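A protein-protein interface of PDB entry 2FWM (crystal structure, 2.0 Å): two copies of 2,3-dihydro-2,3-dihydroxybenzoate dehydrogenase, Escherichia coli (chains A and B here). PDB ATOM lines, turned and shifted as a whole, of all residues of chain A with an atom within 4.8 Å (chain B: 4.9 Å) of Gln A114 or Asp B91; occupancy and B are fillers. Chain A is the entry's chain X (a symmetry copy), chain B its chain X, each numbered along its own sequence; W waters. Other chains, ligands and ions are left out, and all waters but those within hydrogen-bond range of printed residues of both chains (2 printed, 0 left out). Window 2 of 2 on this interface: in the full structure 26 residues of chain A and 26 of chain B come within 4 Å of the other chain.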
ATOM      1  N   PHE A 110      -9.168 -13.887 -33.986  1.00  0.00           N
ATOM      2  CA  PHE A 110      -9.192 -15.350 -33.938  1.00  0.00           C
ATOM      3  C   PHE A 110      -7.914 -15.927 -33.303  1.00  0.00           C
ATOM      4  O   PHE A 110      -7.979 -16.801 -32.434  1.00  0.00           O
ATOM      5  CB  PHE A 110      -9.384 -15.925 -35.348  1.00  0.00           C
ATOM      6  CG  PHE A 110      -9.236 -17.423 -35.422  1.00  0.00           C
ATOM      7  CD1 PHE A 110     -10.179 -18.263 -34.834  1.00  0.00           C
ATOM      8  CD2 PHE A 110      -8.150 -17.996 -36.091  1.00  0.00           C
ATOM      9  CE1 PHE A 110     -10.047 -19.639 -34.908  1.00  0.00           C
ATOM     10  CE2 PHE A 110      -8.017 -19.388 -36.173  1.00  0.00           C
ATOM     11  CZ  PHE A 110      -8.961 -20.202 -35.587  1.00  0.00           C
ATOM     12  N   ASN A 111      -6.761 -15.443 -33.755  1.00  0.00           N
ATOM     13  CA  ASN A 111      -5.476 -15.856 -33.191  1.00  0.00           C
ATOM     14  C   ASN A 111      -5.331 -15.506 -31.703  1.00  0.00           C
ATOM     15  O   ASN A 111      -4.896 -16.338 -30.898  1.00  0.00           O
ATOM     16  CB  ASN A 111      -4.328 -15.266 -34.015  1.00  0.00           C
ATOM     17  CG  ASN A 111      -4.239 -15.872 -35.400  1.00  0.00           C
ATOM     18  OD1 ASN A 111      -4.650 -17.014 -35.616  1.00  0.00           O
ATOM     19  ND2 ASN A 111      -3.692 -15.114 -36.346  1.00  0.00           N
ATOM     20  N   LEU A 112      -5.704 -14.281 -31.342  1.00  0.00           N
ATOM     21  CA  LEU A 112      -5.754 -13.884 -29.937  1.00  0.00           C
ATOM     22  C   LEU A 112      -6.660 -14.792 -29.115  1.00  0.00           C
ATOM     23  O   LEU A 112      -6.260 -15.257 -28.048  1.00  0.00           O
ATOM     24  CB  LEU A 112      -6.201 -12.430 -29.775  1.00  0.00           C
ATOM     25  CG  LEU A 112      -5.134 -11.348 -29.600  1.00  0.00           C
ATOM     26  CD1 LEU A 112      -4.293 -11.600 -28.362  1.00  0.00           C
ATOM     27  CD2 LEU A 112      -4.255 -11.236 -30.855  1.00  0.00           C
ATOM     28  N   PHE A 113      -7.875 -15.036 -29.607  1.00  0.00           N
ATOM     29  CA  PHE A 113      -8.821 -15.925 -28.924  1.00  0.00           C
ATOM     30  C   PHE A 113      -8.261 -17.343 -28.781  1.00  0.00           C
ATOM     31  O   PHE A 113      -8.391 -17.964 -27.728  1.00  0.00           O
ATOM     32  CB  PHE A 113     -10.180 -15.955 -29.640  1.00  0.00           C
ATOM     33  CG  PHE A 113     -10.955 -14.663 -29.553  1.00  0.00           C
ATOM     34  CD1 PHE A 113     -11.677 -14.199 -30.654  1.00  0.00           C
ATOM     35  CD2 PHE A 113     -10.965 -13.910 -28.386  1.00  0.00           C
ATOM     36  CE1 PHE A 113     -12.399 -13.013 -30.587  1.00  0.00           C
ATOM     37  CE2 PHE A 113     -11.682 -12.721 -28.310  1.00  0.00           C
ATOM     38  CZ  PHE A 113     -12.407 -12.274 -29.412  1.00  0.00           C
ATOM     39  N   GLN A 114      -7.614 -17.848 -29.827  1.00  0.00           N
ATOM     40  CA  GLN A 114      -6.989 -19.166 -29.737  1.00  0.00           C
ATOM     41  C   GLN A 114      -5.924 -19.229 -28.631  1.00  0.00           C
ATOM     42  O   GLN A 114      -5.807 -20.247 -27.932  1.00  0.00           O
ATOM     43  CB  GLN A 114      -6.429 -19.623 -31.088  1.00  0.00           C
ATOM     44  CG  GLN A 114      -7.515 -20.024 -32.091  1.00  0.00           C
ATOM     45  CD  GLN A 114      -7.112 -21.194 -32.982  1.00  0.00           C
ATOM     46  OE1 GLN A 114      -6.015 -21.223 -33.542  1.00  0.00           O
ATOM     47  NE2 GLN A 114      -8.012 -22.161 -33.122  1.00  0.00           N
ATOM     48  N   GLN A 115      -5.185 -18.134 -28.447  1.00  0.00           N
ATOM     49  CA  GLN A 115      -4.129 -18.085 -27.424  1.00  0.00           C
ATOM     50  C   GLN A 115      -4.578 -17.703 -26.013  1.00  0.00           C
ATOM     51  O   GLN A 115      -3.879 -18.028 -25.056  1.00  0.00           O
ATOM     52  CB  GLN A 115      -2.964 -17.179 -27.853  1.00  0.00           C
ATOM     53  CG  GLN A 115      -2.253 -17.616 -29.128  1.00  0.00           C
ATOM     54  CD  GLN A 115      -1.798 -19.072 -29.097  1.00  0.00           C
ATOM     55  OE1 GLN A 115      -1.292 -19.560 -28.086  1.00  0.00           O
ATOM     56  NE2 GLN A 115      -1.975 -19.764 -30.209  1.00  0.00           N
ATOM     57  N   THR A 116      -5.716 -17.019 -25.874  1.00  0.00           N
ATOM     58  CA  THR A 116      -6.131 -16.489 -24.565  1.00  0.00           C
ATOM     59  C   THR A 116      -7.360 -17.146 -23.937  1.00  0.00           C
ATOM     60  O   THR A 116      -7.593 -16.974 -22.735  1.00  0.00           O
ATOM     61  CB  THR A 116      -6.389 -14.965 -24.599  1.00  0.00           C
ATOM     62  OG1 THR A 116      -7.465 -14.686 -25.500  1.00  0.00           O
ATOM     63  CG2 THR A 116      -5.133 -14.195 -25.033  1.00  0.00           C
ATOM     64  N   MET A 117      -8.152 -17.884 -24.714  1.00  0.00           N
ATOM     65  CA  MET A 117      -9.392 -18.447 -24.152  1.00  0.00           C
ATOM     66  C   MET A 117      -9.172 -19.344 -22.928  1.00  0.00           C
ATOM     67  O   MET A 117      -9.911 -19.247 -21.948  1.00  0.00           O
ATOM     68  CB  MET A 117     -10.238 -19.141 -25.216  1.00  0.00           C
ATOM     69  CG  MET A 117     -10.980 -18.143 -26.121  1.00  0.00           C
ATOM     70  SD  MET A 117     -11.884 -18.943 -27.452  1.00  0.00           S
ATOM     71  CE  MET A 117     -13.324 -19.556 -26.574  1.00  0.00           C
ATOM     72  N   ASN A 118      -8.149 -20.188 -22.960  1.00  0.00           N
ATOM     73  CA  ASN A 118      -7.918 -21.043 -21.804  1.00  0.00           C
ATOM     74  C   ASN A 118      -7.514 -20.285 -20.545  1.00  0.00           C
ATOM     75  O   ASN A 118      -7.895 -20.677 -19.450  1.00  0.00           O
ATOM     76  CB  ASN A 118      -6.953 -22.181 -22.099  1.00  0.00           C
ATOM     77  CG  ASN A 118      -7.445 -23.493 -21.518  1.00  0.00           C
ATOM     78  OD1 ASN A 118      -8.613 -23.880 -21.719  1.00  0.00           O
ATOM     79  ND2 ASN A 118      -6.577 -24.178 -20.781  1.00  0.00           N
ATOM     80  N   ARG A 121     -10.767 -19.052 -19.112  1.00  0.00           N
ATOM     81  CA  ARG A 121     -11.486 -20.170 -18.489  1.00  0.00           C
ATOM     82  C   ARG A 121     -10.902 -20.497 -17.119  1.00  0.00           C
ATOM     83  O   ARG A 121     -11.628 -20.597 -16.128  1.00  0.00           O
ATOM     84  CB  ARG A 121     -11.438 -21.429 -19.359  1.00  0.00           C
ATOM     85  CG  ARG A 121     -12.311 -21.395 -20.597  1.00  0.00           C
ATOM     86  CD  ARG A 121     -12.358 -22.771 -21.249  1.00  0.00           C
ATOM     87  NE  ARG A 121     -12.838 -22.686 -22.623  1.00  0.00           N
ATOM     88  CZ  ARG A 121     -12.054 -22.653 -23.698  1.00  0.00           C
ATOM     89  NH1 ARG A 121     -10.738 -22.723 -23.578  1.00  0.00           N
ATOM     90  NH2 ARG A 121     -12.601 -22.573 -24.902  1.00  0.00           N
ATOM     91  N   ALA B  89     -14.767 -25.827 -31.014  1.00  0.00           N
ATOM     92  CA  ALA B  89     -14.529 -24.689 -30.114  1.00  0.00           C
ATOM     93  C   ALA B  89     -13.547 -23.718 -30.771  1.00  0.00           C
ATOM     94  O   ALA B  89     -12.666 -24.143 -31.530  1.00  0.00           O
ATOM     95  CB  ALA B  89     -13.993 -25.170 -28.763  1.00  0.00           C
ATOM     96  N   THR B  90     -13.704 -22.422 -30.503  1.00  0.00           N
ATOM     97  CA  THR B  90     -12.872 -21.405 -31.168  1.00  0.00           C
ATOM     98  C   THR B  90     -11.367 -21.685 -31.026  1.00  0.00           C
ATOM     99  O   THR B  90     -10.622 -21.573 -32.001  1.00  0.00           O
ATOM    100  CB  THR B  90     -13.200 -19.968 -30.695  1.00  0.00           C
ATOM    101  OG1 THR B  90     -14.582 -19.685 -30.958  1.00  0.00           O
ATOM    102  CG2 THR B  90     -12.335 -18.929 -31.414  1.00  0.00           C
ATOM    103  N   ASP B  91     -10.933 -22.055 -29.824  1.00  0.00           N
ATOM    104  CA  ASP B  91      -9.506 -22.251 -29.575  1.00  0.00           C
ATOM    105  C   ASP B  91      -8.999 -23.649 -29.969  1.00  0.00           C
ATOM    106  O   ASP B  91      -7.805 -23.944 -29.832  1.00  0.00           O
ATOM    107  CB  ASP B  91      -9.140 -21.904 -28.122  1.00  0.00           C
ATOM    108  CG  ASP B  91      -9.900 -22.735 -27.094  1.00  0.00           C
ATOM    109  OD1 ASP B  91     -11.007 -23.236 -27.398  1.00  0.00           O
ATOM    110  OD2 ASP B  91      -9.386 -22.869 -25.964  1.00  0.00           O
ATOM    111  N   GLN B  92      -9.898 -24.491 -30.475  1.00  0.00           N
ATOM    112  CA  GLN B  92      -9.525 -25.832 -30.942  1.00  0.00           C
ATOM    113  C   GLN B  92      -9.562 -25.987 -32.469  1.00  0.00           C
ATOM    114  O   GLN B  92      -8.947 -26.899 -33.021  1.00  0.00           O
ATOM    115  CB  GLN B  92     -10.387 -26.904 -30.264  1.00  0.00           C
ATOM    116  CG  GLN B  92     -10.180 -26.967 -28.750  1.00  0.00           C
ATOM    117  CD  GLN B  92     -10.702 -28.247 -28.134  1.00  0.00           C
ATOM    118  OE1 GLN B  92     -10.045 -29.291 -28.195  1.00  0.00           O
ATOM    119  NE2 GLN B  92     -11.882 -28.173 -27.521  1.00  0.00           N
ATOM    120  N   LEU B  93     -10.282 -25.091 -33.142  1.00  0.00           N
ATOM    121  CA  LEU B  93     -10.391 -25.132 -34.597  1.00  0.00           C
ATOM    122  C   LEU B  93      -9.022 -25.025 -35.279  1.00  0.00           C
ATOM    123  O   LEU B  93      -8.202 -24.173 -34.916  1.00  0.00           O
ATOM    124  CB  LEU B  93     -11.317 -24.010 -35.079  1.00  0.00           C
ATOM    125  CG  LEU B  93     -11.782 -24.083 -36.533  1.00  0.00           C
ATOM    126  CD1 LEU B  93     -12.870 -25.138 -36.701  1.00  0.00           C
ATOM    127  CD2 LEU B  93     -12.286 -22.712 -36.966  1.00  0.00           C
ATOM    128  N   LYS B  95      -6.208 -24.196 -38.182  1.00  0.00           N
ATOM    129  CA  LYS B  95      -6.023 -23.085 -39.108  1.00  0.00           C
ATOM    130  C   LYS B  95      -6.480 -23.412 -40.526  1.00  0.00           C
ATOM    131  O   LYS B  95      -6.992 -22.541 -41.227  1.00  0.00           O
ATOM    132  CB  LYS B  95      -4.583 -22.560 -39.062  1.00  0.00           C
ATOM    133  CG  LYS B  95      -4.361 -21.616 -37.866  1.00  0.00           C
ATOM    134  CD  LYS B  95      -2.908 -21.563 -37.426  1.00  0.00           C
ATOM    135  CE  LYS B  95      -2.850 -21.570 -35.907  1.00  0.00           C
ATOM    136  NZ  LYS B  95      -1.499 -21.280 -35.360  1.00  0.00           N
HETATM  137  O   HOH W   1      -5.482 -22.913 -29.080  1.00  0.00           O
HETATM  138  O   HOH W   2      -6.858 -21.060 -25.369  1.00  0.00           O
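The backbone carbonyl oxygen (O) of Thr B90 is in hydrogen-bond range of the side-chain amide nitrogen (NE2) of Gln A114. NH1 of Arg A121 lies within salt-bridge range of OD2 of Asp B91, 2.7 Å away. O of Leu B93 lies within hydrogen-bond range of NE2 of Gln A114, 2.7 Å away.
The side-chain amide oxygen (OD1) of Asn A118 is in hydrogen-bond range of the guanidinium group (NH1) of Arg A121, 3.1 Å away.
CE1 of Phe A110 touches O of Thr B90 (3.5 Å). Gln A114 touches Asp B91 (NE2 to C, 3.6 Å). Gln B92 touches Gln A114. Lys B95 touches Gln A114 (CE to OE1, 3.97 Å). Thr B90 touches Met A117 (CB to SD, 3.6 Å). Asp B91 touches Met A117 (OD2 to CB, 3.9 Å).
Of the printed residues of chain B, Phe A110 touches Thr B90. Leu A112 touches none of the printed residues of chain B. Phe A113 touches none of the printed residues of chain B. Printed residues of chain B within 4 Å of Gln A114: Thr B90, Asp B91, Gln B92, Leu B93 and Lys B95. Printed residues of chain B within 4 Å of Arg A121: Asp B91. Printed residues of chain A within 4 Å of Thr B90: Phe A110 (3.5 Å), Gln A114 (2.9 Å) and Met A117 (3.6 Å). Asp B91 touches just these residues of chain A: Gln A114 (3.6 Å), Met A117 (3.9 Å) and Arg A121 (2.7 Å). Of the printed residues of chain A, Gln B92 touches Gln A114 (3.999 Å). Of the printed residues of chain A, Lys B95 touches Gln A114 (3.97 Å).
Of the 10 printed residues of chain A, 4 touch a printed residue of chain B. Hydrophobic or aromatic side chains of chain A within 4 Å of the printed part of chain B: Phe A110 and Met A117. Along chain B the printed residues that touch a printed residue of chain A span positions 90 to 95. Among the printed residues, 9 pairs touch across the chains. Among the printed residues, Asp or Glu carboxylates within 4 Å of a Lys or Arg side-chain nitrogen of the other chain: Arg A121 with Asp B91 (2.7 Å).
No position is printed for both chains. Of the 9 pairs that touch across the chains among the printed residues, none has its exchanged pair printed and touching as well.
Water W1 lies within hydrogen-bond range of O of Asp B91 (2.7 Å) and O of Gln A114 (2.9 Å). Water W2 lies within hydrogen-bond range of the backbone NH (N) of Asn A118 (2.9 Å), the backbone carbonyl oxygen (O) of Gln A114 (2.9 Å), the side-chain carboxylate (OD2) of Asp B91 (3.2 Å) and the backbone NH (N) of Met A117 (3.5 Å).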
